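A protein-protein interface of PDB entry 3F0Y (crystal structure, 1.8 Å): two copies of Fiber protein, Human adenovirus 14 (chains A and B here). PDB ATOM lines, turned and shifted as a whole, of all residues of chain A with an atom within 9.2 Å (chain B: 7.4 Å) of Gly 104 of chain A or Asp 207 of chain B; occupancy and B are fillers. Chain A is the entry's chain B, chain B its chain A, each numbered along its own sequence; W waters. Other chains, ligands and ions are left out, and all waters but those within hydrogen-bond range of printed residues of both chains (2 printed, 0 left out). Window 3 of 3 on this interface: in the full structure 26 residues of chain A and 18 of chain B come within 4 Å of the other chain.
Among the printed residues, merely in contact across the chains: Gly 104 of chain A with Asp 207 of chain B, Val 21 of chain A with Ile 204 of chain B, Gln 105 of chain A with Thr 123 of chain B, Trp 18 of chain A with Ala 50 of chain B, Val 21 of chain A with Thr 123 of chain B, Lys 102 of chain A with Ala 50 of chain B, Gln 105 of chain A with Ile 204 of chain B and Trp 18 of chain A with Ile 204 of chain B.
The side-chain hydroxyl (OG1) of Thr 16 of chain A is in hydrogen-bond range of the backbone NH (N) of Ala 50 of chain B (2.9 Å). The side-chain hydroxyl (OG) of Ser 121 of chain B sits at hydrogen-bond distance from the side-chain amide nitrogen (NE2) of Gln 105 of chain A. The backbone carbonyl oxygen of Arg 205 of chain B lies close to the side-chain amide oxygen of Gln 105 of chain A (3.1 Å). The side-chain carboxylate of Asp 207 of chain B lies within salt-bridge range of the side-chain amino group of Lys 102 of chain A (2.8 Å). OD1 of Asp 207 of chain B lies close to OE1 of Gln 105 of chain A (2.8 Å).
Of the printed residues of chain B, Thr 16 of chain A touches Ala 50. Thr 44 of chain A touches none of the printed residues of chain B. Of the printed residues of chain B, Lys 102 of chain A touches Ala 50 and Asp 207. Printed residues of chain A within 4 Å of Ser 121 of chain B: Gln 105 (2.6 Å). Of the printed residues of chain A, Arg 205 of chain B touches Gln 105 (3.1 Å). No residue of chain A comes within 4 Å of Glu 206 of chain B. Asp 207 of chain B touches just these residues of chain A: Lys 102 (2.8 Å), Gly 104 (3.2 Å) and Gln 105 (2.8 Å). Asp 208 of chain B touches none of the printed residues of chain A. The nearest residue of chain A that does not touch Asp 207 of chain B is Ser 103 of chain A (5.6 Å).
Of the 17 printed residues of chain A, 6 touch a printed residue of chain B. Printed residues of chain A that touch a printed residue of chain B: Thr 16, Trp 18, Val 21, Lys 102, Gly 104 and Gln 105. Hydrophobic or aromatic side chains of chain A that line the printed part of chain B: Trp 18 and Val 21. Of the 16 printed residues of chain B, 6 touch a printed residue of chain A. Printed residues of chain B that touch a printed residue of chain A: Ala 50, Ser 121, Thr 123, Ile 204, Arg 205 and Asp 207. Among the printed residues, 13 pairs touch across the chains. Among the printed residues, Asp or Glu carboxylates within 4 Å of a Lys or Arg side-chain nitrogen of the other chain: Lys 102 of chain A with Asp 207 of chain B.
No position is printed for both chains.
Water W2 lies within hydrogen-bond range of NZ of Lys 102 of chain A (2.7 Å), O of Arg 205 of chain B (2.8 Å) and O of Ala 50 of chain B (2.9 Å). Water W1 lies within hydrogen-bond range of the side-chain carboxylate of Asp 207 of chain B, the guanidinium group of Arg 205 of chain B, the backbone carbonyl oxygen of Glu 206 of chain B and the side-chain amino group of Lys 102 of chain A.
O of Ala 50 of chain B is in hydrogen-bond range of N of Arg 205 of chain B (3.1 Å). O of Asp 207 of chain B is in hydrogen-bond range of NZ of Lys 116 of chain B, 2.6 Å away. OG of Ser 121 of chain B is in hydrogen-bond range of N of Thr 123 of chain B, at 3.0 Å. N of Trp 18 of chain A sits at hydrogen-bond distance from O of Asn 100 of chain A (2.8 Å). The indole nitrogen (NE1) of Trp 18 of chain A is in hydrogen-bond range of the backbone carbonyl oxygen (O) of Asn 106 of chain A (3.1 Å). The backbone carbonyl oxygen (O) of Gly 104 of chain A lies within hydrogen-bond range of the side-chain amino group (NZ) of Lys 102 of chain A (2.7 Å).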
ATOM      1  N   ASP A  11       3.010 -16.358  17.934  1.00  0.00           N
ATOM      2  CA  ASP A  11       2.999 -14.886  18.183  1.00  0.00           C
ATOM      3  C   ASP A  11       4.159 -14.221  17.446  1.00  0.00           C
ATOM      4  O   ASP A  11       5.314 -14.361  17.846  1.00  0.00           O
ATOM      5  CB  ASP A  11       3.090 -14.604  19.686  1.00  0.00           C
ATOM      6  CG  ASP A  11       3.053 -13.116  20.015  1.00  0.00           C
ATOM      7  OD1 ASP A  11       2.475 -12.333  19.228  1.00  0.00           O
ATOM      8  OD2 ASP A  11       3.598 -12.733  21.073  1.00  0.00           O
ATOM      9  N   ASN A  13       4.989 -11.155  17.328  1.00  0.00           N
ATOM     10  CA  ASN A  13       5.603 -10.103  18.148  1.00  0.00           C
ATOM     11  C   ASN A  13       6.957 -10.487  18.756  1.00  0.00           C
ATOM     12  O   ASN A  13       7.814  -9.624  18.954  1.00  0.00           O
ATOM     13  CB  ASN A  13       4.650  -9.677  19.273  1.00  0.00           C
ATOM     14  CG  ASN A  13       3.452  -8.883  18.766  1.00  0.00           C
ATOM     15  OD1 ASN A  13       3.571  -8.066  17.855  1.00  0.00           O
ATOM     16  ND2 ASN A  13       2.291  -9.118  19.367  1.00  0.00           N
ATOM     17  N   THR A  16      10.530  -9.884  16.921  1.00  0.00           N
ATOM     18  CA  THR A  16      11.149  -8.569  16.964  1.00  0.00           C
ATOM     19  C   THR A  16      11.742  -8.312  18.347  1.00  0.00           C
ATOM     20  O   THR A  16      11.115  -8.601  19.364  1.00  0.00           O
ATOM     21  CB  THR A  16      10.128  -7.461  16.648  1.00  0.00           C
ATOM     22  OG1 THR A  16       9.657  -7.614  15.304  1.00  0.00           O
ATOM     23  CG2 THR A  16      10.755  -6.076  16.812  1.00  0.00           C
ATOM     24  N   TRP A  18      13.333  -4.869  19.962  1.00  0.00           N
ATOM     25  CA  TRP A  18      13.484  -3.474  19.564  1.00  0.00           C
ATOM     26  C   TRP A  18      13.364  -2.474  20.707  1.00  0.00           C
ATOM     27  O   TRP A  18      13.101  -2.838  21.856  1.00  0.00           O
ATOM     28  CB  TRP A  18      12.505  -3.146  18.418  1.00  0.00           C
ATOM     29  CG  TRP A  18      11.066  -2.941  18.806  1.00  0.00           C
ATOM     30  CD1 TRP A  18      10.453  -3.341  19.958  1.00  0.00           C
ATOM     31  CD2 TRP A  18      10.052  -2.310  18.013  1.00  0.00           C
ATOM     32  NE1 TRP A  18       9.131  -2.977  19.943  1.00  0.00           N
ATOM     33  CE2 TRP A  18       8.855  -2.349  18.757  1.00  0.00           C
ATOM     34  CE3 TRP A  18      10.042  -1.709  16.747  1.00  0.00           C
ATOM     35  CZ2 TRP A  18       7.659  -1.807  18.281  1.00  0.00           C
ATOM     36  CZ3 TRP A  18       8.853  -1.172  16.274  1.00  0.00           C
ATOM     37  CH2 TRP A  18       7.678  -1.225  17.039  1.00  0.00           C
ATOM     38  N   THR A  19      13.586  -1.211  20.359  1.00  0.00           N
ATOM     39  CA  THR A  19      13.552  -0.092  21.288  1.00  0.00           C
ATOM     40  C   THR A  19      12.159   0.518  21.406  1.00  0.00           C
ATOM     41  O   THR A  19      11.917   1.369  22.263  1.00  0.00           O
ATOM     42  CB  THR A  19      14.491   1.014  20.791  1.00  0.00           C
ATOM     43  OG1 THR A  19      14.142   1.353  19.441  1.00  0.00           O
ATOM     44  CG2 THR A  19      15.934   0.543  20.832  1.00  0.00           C
ATOM     45  N   GLY A  20      11.246   0.089  20.539  1.00  0.00           N
ATOM     46  CA  GLY A  20       9.971   0.760  20.379  1.00  0.00           C
ATOM     47  C   GLY A  20      10.149   1.936  19.438  1.00  0.00           C
ATOM     48  O   GLY A  20      11.275   2.300  19.088  1.00  0.00           O
ATOM     49  N   VAL A  21       9.033   2.526  19.028  1.00  0.00           N
ATOM     50  CA  VAL A  21       9.050   3.636  18.086  1.00  0.00           C
ATOM     51  C   VAL A  21       9.059   4.961  18.834  1.00  0.00           C
ATOM     52  O   VAL A  21       8.291   5.151  19.778  1.00  0.00           O
ATOM     53  CB  VAL A  21       7.823   3.596  17.156  1.00  0.00           C
ATOM     54  CG1 VAL A  21       7.804   4.817  16.247  1.00  0.00           C
ATOM     55  CG2 VAL A  21       7.823   2.313  16.342  1.00  0.00           C
ATOM     56  N   THR A  44      15.749  -1.951  15.650  1.00  0.00           N
ATOM     57  CA  THR A  44      14.823  -3.063  15.498  1.00  0.00           C
ATOM     58  C   THR A  44      15.582  -4.276  14.965  1.00  0.00           C
ATOM     59  O   THR A  44      16.207  -4.212  13.909  1.00  0.00           O
ATOM     60  CB  THR A  44      13.671  -2.689  14.549  1.00  0.00           C
ATOM     61  OG1 THR A  44      13.019  -1.509  15.037  1.00  0.00           O
ATOM     62  CG2 THR A  44      12.657  -3.823  14.437  1.00  0.00           C
ATOM     63  N   ASN A 100      12.981  -5.009  24.070  1.00  0.00           N
ATOM     64  CA  ASN A 100      11.949  -6.010  24.301  1.00  0.00           C
ATOM     65  C   ASN A 100      11.203  -6.269  23.003  1.00  0.00           C
ATOM     66  O   ASN A 100      11.576  -5.739  21.955  1.00  0.00           O
ATOM     67  CB  ASN A 100      11.001  -5.566  25.423  1.00  0.00           C
ATOM     68  CG  ASN A 100      10.473  -6.736  26.245  1.00  0.00           C
ATOM     69  OD1 ASN A 100       9.822  -7.636  25.714  1.00  0.00           O
ATOM     70  ND2 ASN A 100      10.746  -6.722  27.548  1.00  0.00           N
ATOM     71  N   HIS A 101      10.165  -7.094  23.071  1.00  0.00           N
ATOM     72  CA  HIS A 101       9.409  -7.478  21.888  1.00  0.00           C
ATOM     73  C   HIS A 101       8.469  -6.380  21.432  1.00  0.00           C
ATOM     74  O   HIS A 101       8.271  -5.387  22.128  1.00  0.00           O
ATOM     75  CB  HIS A 101       8.621  -8.758  22.160  1.00  0.00           C
ATOM     76  CG  HIS A 101       9.490  -9.945  22.413  1.00  0.00           C
ATOM     77  ND1 HIS A 101      10.505 -10.315  21.558  1.00  0.00           N
ATOM     78  CD2 HIS A 101       9.501 -10.845  23.424  1.00  0.00           C
ATOM     79  CE1 HIS A 101      11.103 -11.393  22.030  1.00  0.00           C
ATOM     80  NE2 HIS A 101      10.511 -11.734  23.161  1.00  0.00           N
ATOM     81  N   LYS A 102       7.901  -6.571  20.246  1.00  0.00           N
ATOM     82  CA  LYS A 102       6.919  -5.644  19.708  1.00  0.00           C
ATOM     83  C   LYS A 102       5.641  -5.709  20.534  1.00  0.00           C
ATOM     84  O   LYS A 102       5.115  -6.790  20.798  1.00  0.00           O
ATOM     85  CB  LYS A 102       6.613  -5.967  18.241  1.00  0.00           C
ATOM     86  CG  LYS A 102       5.629  -5.010  17.579  1.00  0.00           C
ATOM     87  CD  LYS A 102       5.323  -5.435  16.152  1.00  0.00           C
ATOM     88  CE  LYS A 102       4.052  -4.782  15.637  1.00  0.00           C
ATOM     89  NZ  LYS A 102       4.145  -3.297  15.617  1.00  0.00           N
ATOM     90  N   SER A 103       5.170  -4.542  20.958  1.00  0.00           N
ATOM     91  CA  SER A 103       3.851  -4.406  21.557  1.00  0.00           C
ATOM     92  C   SER A 103       3.230  -3.155  20.957  1.00  0.00           C
ATOM     93  O   SER A 103       3.304  -2.066  21.527  1.00  0.00           O
ATOM     94  CB  SER A 103       3.945  -4.311  23.080  1.00  0.00           C
ATOM     95  OG  SER A 103       2.657  -4.359  23.664  1.00  0.00           O
ATOM     96  N   GLY A 104       2.639  -3.322  19.780  1.00  0.00           N
ATOM     97  CA  GLY A 104       2.185  -2.188  18.990  1.00  0.00           C
ATOM     98  C   GLY A 104       3.393  -1.396  18.529  1.00  0.00           C
ATOM     99  O   GLY A 104       4.337  -1.964  17.980  1.00  0.00           O
ATOM    100  N   GLN A 105       3.373  -0.089  18.778  1.00  0.00           N
ATOM    101  CA  GLN A 105       4.494   0.792  18.445  1.00  0.00           C
ATOM    102  C   GLN A 105       5.506   0.894  19.589  1.00  0.00           C
ATOM    103  O   GLN A 105       6.493   1.622  19.483  1.00  0.00           O
ATOM    104  CB  GLN A 105       3.975   2.191  18.093  1.00  0.00           C
ATOM    105  CG  GLN A 105       2.986   2.215  16.939  1.00  0.00           C
ATOM    106  CD  GLN A 105       3.601   1.749  15.634  1.00  0.00           C
ATOM    107  OE1 GLN A 105       3.145   0.780  15.028  1.00  0.00           O
ATOM    108  NE2 GLN A 105       4.652   2.430  15.202  1.00  0.00           N
ATOM    109  N   ASN A 106       5.260   0.155  20.670  1.00  0.00           N
ATOM    110  CA  ASN A 106       6.074   0.220  21.877  1.00  0.00           C
ATOM    111  C   ASN A 106       6.767  -1.104  22.161  1.00  0.00           C
ATOM    112  O   ASN A 106       6.545  -2.092  21.466  1.00  0.00           O
ATOM    113  CB  ASN A 106       5.185   0.587  23.065  1.00  0.00           C
ATOM    114  CG  ASN A 106       4.464   1.902  22.867  1.00  0.00           C
ATOM    115  OD1 ASN A 106       5.028   2.858  22.335  1.00  0.00           O
ATOM    116  ND2 ASN A 106       3.207   1.958  23.294  1.00  0.00           N
ATOM    117  N   MET A 107       7.613  -1.111  23.187  1.00  0.00           N
ATOM    118  CA  MET A 107       8.227  -2.338  23.670  1.00  0.00           C
ATOM    119  C   MET A 107       7.250  -3.083  24.565  1.00  0.00           C
ATOM    120  O   MET A 107       6.494  -2.461  25.316  1.00  0.00           O
ATOM    121  CB  MET A 107       9.487  -2.032  24.476  1.00  0.00           C
ATOM    122  CG  MET A 107      10.610  -1.439  23.667  1.00  0.00           C
ATOM    123  SD  MET A 107      12.088  -1.228  24.664  1.00  0.00           S
ATOM    124  CE  MET A 107      11.638   0.205  25.636  1.00  0.00           C
ATOM    125  N   ALA A 108       7.270  -4.411  24.483  1.00  0.00           N
ATOM    126  CA  ALA A 108       6.584  -5.249  25.464  1.00  0.00           C
ATOM    127  C   ALA A 108       7.288  -5.075  26.812  1.00  0.00           C
ATOM    128  O   ALA A 108       8.400  -4.544  26.872  1.00  0.00           O
ATOM    129  CB  ALA A 108       6.598  -6.705  25.031  1.00  0.00           C
ATOM    130  N   ALA B  50       8.352  -6.342  13.034  1.00  0.00           N
ATOM    131  CA  ALA B  50       7.848  -4.978  13.210  1.00  0.00           C
ATOM    132  C   ALA B  50       8.003  -4.120  11.952  1.00  0.00           C
ATOM    133  O   ALA B  50       7.499  -2.998  11.904  1.00  0.00           O
ATOM    134  CB  ALA B  50       8.554  -4.310  14.378  1.00  0.00           C
ATOM    135  N   SER B  84      -7.797   4.837   5.301  1.00  0.00           N
ATOM    136  CA  SER B  84      -7.652   4.402   6.694  1.00  0.00           C
ATOM    137  C   SER B  84      -7.645   2.879   6.890  1.00  0.00           C
ATOM    138  O   SER B  84      -7.189   2.395   7.925  1.00  0.00           O
ATOM    139  CB  SER B  84      -8.755   5.023   7.559  1.00  0.00           C
ATOM    140  OG  SER B  84     -10.038   4.612   7.119  1.00  0.00           O
ATOM    141  N   LYS B 116      -4.006  -2.745   6.684  1.00  0.00           N
ATOM    142  CA  LYS B 116      -3.511  -1.596   7.439  1.00  0.00           C
ATOM    143  C   LYS B 116      -2.111  -1.823   8.018  1.00  0.00           C
ATOM    144  O   LYS B 116      -1.330  -0.880   8.140  1.00  0.00           O
ATOM    145  CB  LYS B 116      -4.489  -1.241   8.562  1.00  0.00           C
ATOM    146  CG  LYS B 116      -4.339   0.176   9.077  1.00  0.00           C
ATOM    147  CD  LYS B 116      -5.518   0.591   9.947  1.00  0.00           C
ATOM    148  CE  LYS B 116      -5.314   0.207  11.392  1.00  0.00           C
ATOM    149  NZ  LYS B 116      -4.343   1.110  12.069  1.00  0.00           N
ATOM    150  N   SER B 117      -1.791  -3.069   8.358  1.00  0.00           N
ATOM    151  CA  SER B 117      -0.484  -3.391   8.934  1.00  0.00           C
ATOM    152  C   SER B 117       0.642  -3.522   7.898  1.00  0.00           C
ATOM    153  O   SER B 117       1.770  -3.846   8.258  1.00  0.00           O
ATOM    154  CB  SER B 117      -0.571  -4.657   9.789  1.00  0.00           C
ATOM    155  OG  SER B 117      -1.216  -5.702   9.092  1.00  0.00           O
ATOM    156  N   PHE B 118       0.340  -3.280   6.625  1.00  0.00           N
ATOM    157  CA  PHE B 118       1.375  -3.096   5.605  1.00  0.00           C
ATOM    158  C   PHE B 118       1.793  -1.628   5.500  1.00  0.00           C
ATOM    159  O   PHE B 118       2.791  -1.313   4.856  1.00  0.00           O
ATOM    160  CB  PHE B 118       0.887  -3.570   4.233  1.00  0.00           C
ATOM    161  CG  PHE B 118       0.811  -5.061   4.096  1.00  0.00           C
ATOM    162  CD1 PHE B 118      -0.378  -5.737   4.344  1.00  0.00           C
ATOM    163  CD2 PHE B 118       1.924  -5.789   3.705  1.00  0.00           C
ATOM    164  CE1 PHE B 118      -0.448  -7.119   4.209  1.00  0.00           C
ATOM    165  CE2 PHE B 118       1.860  -7.166   3.570  1.00  0.00           C
ATOM    166  CZ  PHE B 118       0.675  -7.833   3.821  1.00  0.00           C
ATOM    167  N   MET B 119       1.027  -0.739   6.129  1.00  0.00           N
ATOM    168  CA  MET B 119       1.216   0.699   5.966  1.00  0.00           C
ATOM    169  C   MET B 119       2.381   1.233   6.787  1.00  0.00           C
ATOM    170  O   MET B 119       2.731   0.658   7.816  1.00  0.00           O
ATOM    171  CB  MET B 119      -0.052   1.446   6.383  1.00  0.00           C
ATOM    172  CG  MET B 119      -1.276   1.118   5.550  1.00  0.00           C
ATOM    173  SD  MET B 119      -1.076   1.638   3.840  1.00  0.00           S
ATOM    174  CE  MET B 119      -0.510   0.123   3.078  1.00  0.00           C
ATOM    175  N   PRO B 120       2.975   2.354   6.339  1.00  0.00           N
ATOM    176  CA  PRO B 120       3.990   3.022   7.150  1.00  0.00           C
ATOM    177  C   PRO B 120       3.375   3.618   8.411  1.00  0.00           C
ATOM    178  O   PRO B 120       2.366   4.323   8.336  1.00  0.00           O
ATOM    179  CB  PRO B 120       4.516   4.125   6.224  1.00  0.00           C
ATOM    180  CG  PRO B 120       3.414   4.380   5.270  1.00  0.00           C
ATOM    181  CD  PRO B 120       2.738   3.060   5.067  1.00  0.00           C
ATOM    182  N   SER B 121       3.975   3.310   9.558  1.00  0.00           N
ATOM    183  CA  SER B 121       3.482   3.774  10.848  1.00  0.00           C
ATOM    184  C   SER B 121       3.372   5.294  10.901  1.00  0.00           C
ATOM    185  O   SER B 121       4.325   6.002  10.580  1.00  0.00           O
ATOM    186  CB  SER B 121       4.408   3.293  11.972  1.00  0.00           C
ATOM    187  OG  SER B 121       4.135   3.973  13.183  1.00  0.00           O
ATOM    188  N   THR B 122       2.207   5.790  11.309  1.00  0.00           N
ATOM    189  CA  THR B 122       2.023   7.223  11.539  1.00  0.00           C
ATOM    190  C   THR B 122       2.724   7.663  12.825  1.00  0.00           C
ATOM    191  O   THR B 122       2.951   8.853  13.034  1.00  0.00           O
ATOM    192  CB  THR B 122       0.533   7.611  11.601  1.00  0.00           C
ATOM    193  OG1 THR B 122      -0.133   6.818  12.590  1.00  0.00           O
ATOM    194  CG2 THR B 122      -0.130   7.397  10.247  1.00  0.00           C
ATOM    195  N   THR B 123       3.061   6.703  13.686  1.00  0.00           N
ATOM    196  CA  THR B 123       3.854   6.981  14.878  1.00  0.00           C
ATOM    197  C   THR B 123       5.324   7.160  14.511  1.00  0.00           C
ATOM    198  O   THR B 123       5.977   8.058  15.023  1.00  0.00           O
ATOM    199  CB  THR B 123       3.714   5.866  15.932  1.00  0.00           C
ATOM    200  OG1 THR B 123       2.327   5.661  16.225  1.00  0.00           O
ATOM    201  CG2 THR B 123       4.447   6.238  17.213  1.00  0.00           C
ATOM    202  N   TYR B 171      -2.443   7.145   4.674  1.00  0.00           N
ATOM    203  CA  TYR B 171      -1.047   6.719   4.536  1.00  0.00           C
ATOM    204  C   TYR B 171      -0.503   7.066   3.160  1.00  0.00           C
ATOM    205  O   TYR B 171      -1.238   7.040   2.170  1.00  0.00           O
ATOM    206  CB  TYR B 171      -0.916   5.214   4.779  1.00  0.00           C
ATOM    207  CG  TYR B 171      -1.563   4.760   6.064  1.00  0.00           C
ATOM    208  CD1 TYR B 171      -2.855   4.239   6.069  1.00  0.00           C
ATOM    209  CD2 TYR B 171      -0.896   4.878   7.278  1.00  0.00           C
ATOM    210  CE1 TYR B 171      -3.457   3.830   7.249  1.00  0.00           C
ATOM    211  CE2 TYR B 171      -1.490   4.474   8.463  1.00  0.00           C
ATOM    212  CZ  TYR B 171      -2.770   3.953   8.443  1.00  0.00           C
ATOM    213  OH  TYR B 171      -3.356   3.555   9.618  1.00  0.00           O
ATOM    214  N   ILE B 204       8.970   0.941   9.588  1.00  0.00           N
ATOM    215  CA  ILE B 204       8.217   0.448  10.730  1.00  0.00           C
ATOM    216  C   ILE B 204       6.746   0.469  10.354  1.00  0.00           C
ATOM    217  O   ILE B 204       6.217   1.501   9.940  1.00  0.00           O
ATOM    218  CB  ILE B 204       8.455   1.310  11.981  1.00  0.00           C
ATOM    219  CG1 ILE B 204       9.923   1.224  12.411  1.00  0.00           C
ATOM    220  CG2 ILE B 204       7.543   0.864  13.119  1.00  0.00           C
ATOM    221  CD1 ILE B 204      10.315   2.243  13.452  1.00  0.00           C
ATOM    222  N   ARG B 205       6.086  -0.673  10.488  1.00  0.00           N
ATOM    223  CA  ARG B 205       4.724  -0.784   9.994  1.00  0.00           C
ATOM    224  C   ARG B 205       3.673  -0.378  11.022  1.00  0.00           C
ATOM    225  O   ARG B 205       3.884  -0.466  12.235  1.00  0.00           O
ATOM    226  CB  ARG B 205       4.443  -2.177   9.421  1.00  0.00           C
ATOM    227  CG  ARG B 205       4.576  -3.350  10.368  1.00  0.00           C
ATOM    228  CD  ARG B 205       4.550  -4.645   9.563  1.00  0.00           C
ATOM    229  NE  ARG B 205       4.559  -5.860  10.373  1.00  0.00           N
ATOM    230  CZ  ARG B 205       3.533  -6.293  11.105  1.00  0.00           C
ATOM    231  NH1 ARG B 205       2.392  -5.616  11.154  1.00  0.00           N
ATOM    232  NH2 ARG B 205       3.649  -7.416  11.801  1.00  0.00           N
ATOM    233  N   GLU B 206       2.551   0.105  10.499  1.00  0.00           N
ATOM    234  CA  GLU B 206       1.387   0.471  11.292  1.00  0.00           C
ATOM    235  C   GLU B 206       0.810  -0.792  11.922  1.00  0.00           C
ATOM    236  O   GLU B 206       1.035  -1.895  11.425  1.00  0.00           O
ATOM    237  CB  GLU B 206       0.356   1.142  10.372  1.00  0.00           C
ATOM    238  CG  GLU B 206      -0.939   1.629  11.021  1.00  0.00           C
ATOM    239  CD  GLU B 206      -0.824   2.995  11.672  1.00  0.00           C
ATOM    240  OE1 GLU B 206       0.297   3.425  12.010  1.00  0.00           O
ATOM    241  OE2 GLU B 206      -1.875   3.644  11.851  1.00  0.00           O
ATOM    242  N   ASP B 207       0.090  -0.629  13.027  1.00  0.00           N
ATOM    243  CA  ASP B 207      -0.627  -1.741  13.648  1.00  0.00           C
ATOM    244  C   ASP B 207      -2.056  -1.804  13.127  1.00  0.00           C
ATOM    245  O   ASP B 207      -2.640  -0.780  12.775  1.00  0.00           O
ATOM    246  CB  ASP B 207      -0.628  -1.587  15.163  1.00  0.00           C
ATOM    247  CG  ASP B 207       0.763  -1.650  15.748  1.00  0.00           C
ATOM    248  OD1 ASP B 207       1.170  -0.679  16.411  1.00  0.00           O
ATOM    249  OD2 ASP B 207       1.456  -2.669  15.532  1.00  0.00           O
ATOM    250  N   ASP B 208      -2.610  -3.012  13.083  1.00  0.00           N
ATOM    251  CA  ASP B 208      -3.992  -3.215  12.641  1.00  0.00           C
ATOM    252  C   ASP B 208      -4.982  -2.613  13.632  1.00  0.00           C
ATOM    253  O   ASP B 208      -4.680  -2.459  14.816  1.00  0.00           O
ATOM    254  CB  ASP B 208      -4.286  -4.705  12.457  1.00  0.00           C
ATOM    255  CG  ASP B 208      -3.602  -5.284  11.236  1.00  0.00           C
ATOM    256  OD1 ASP B 208      -3.890  -4.811  10.111  1.00  0.00           O
ATOM    257  OD2 ASP B 208      -2.780  -6.212  11.400  1.00  0.00           O
ATOM    258  OXT ASP B 208      -6.105  -2.263  13.265  1.00  0.00           O
HETATM  259  O   HOH W   1       2.124  -3.788  13.153  1.00  0.00           O
HETATM  260  O   HOH W   2       5.634  -1.933  13.847  1.00  0.00           O
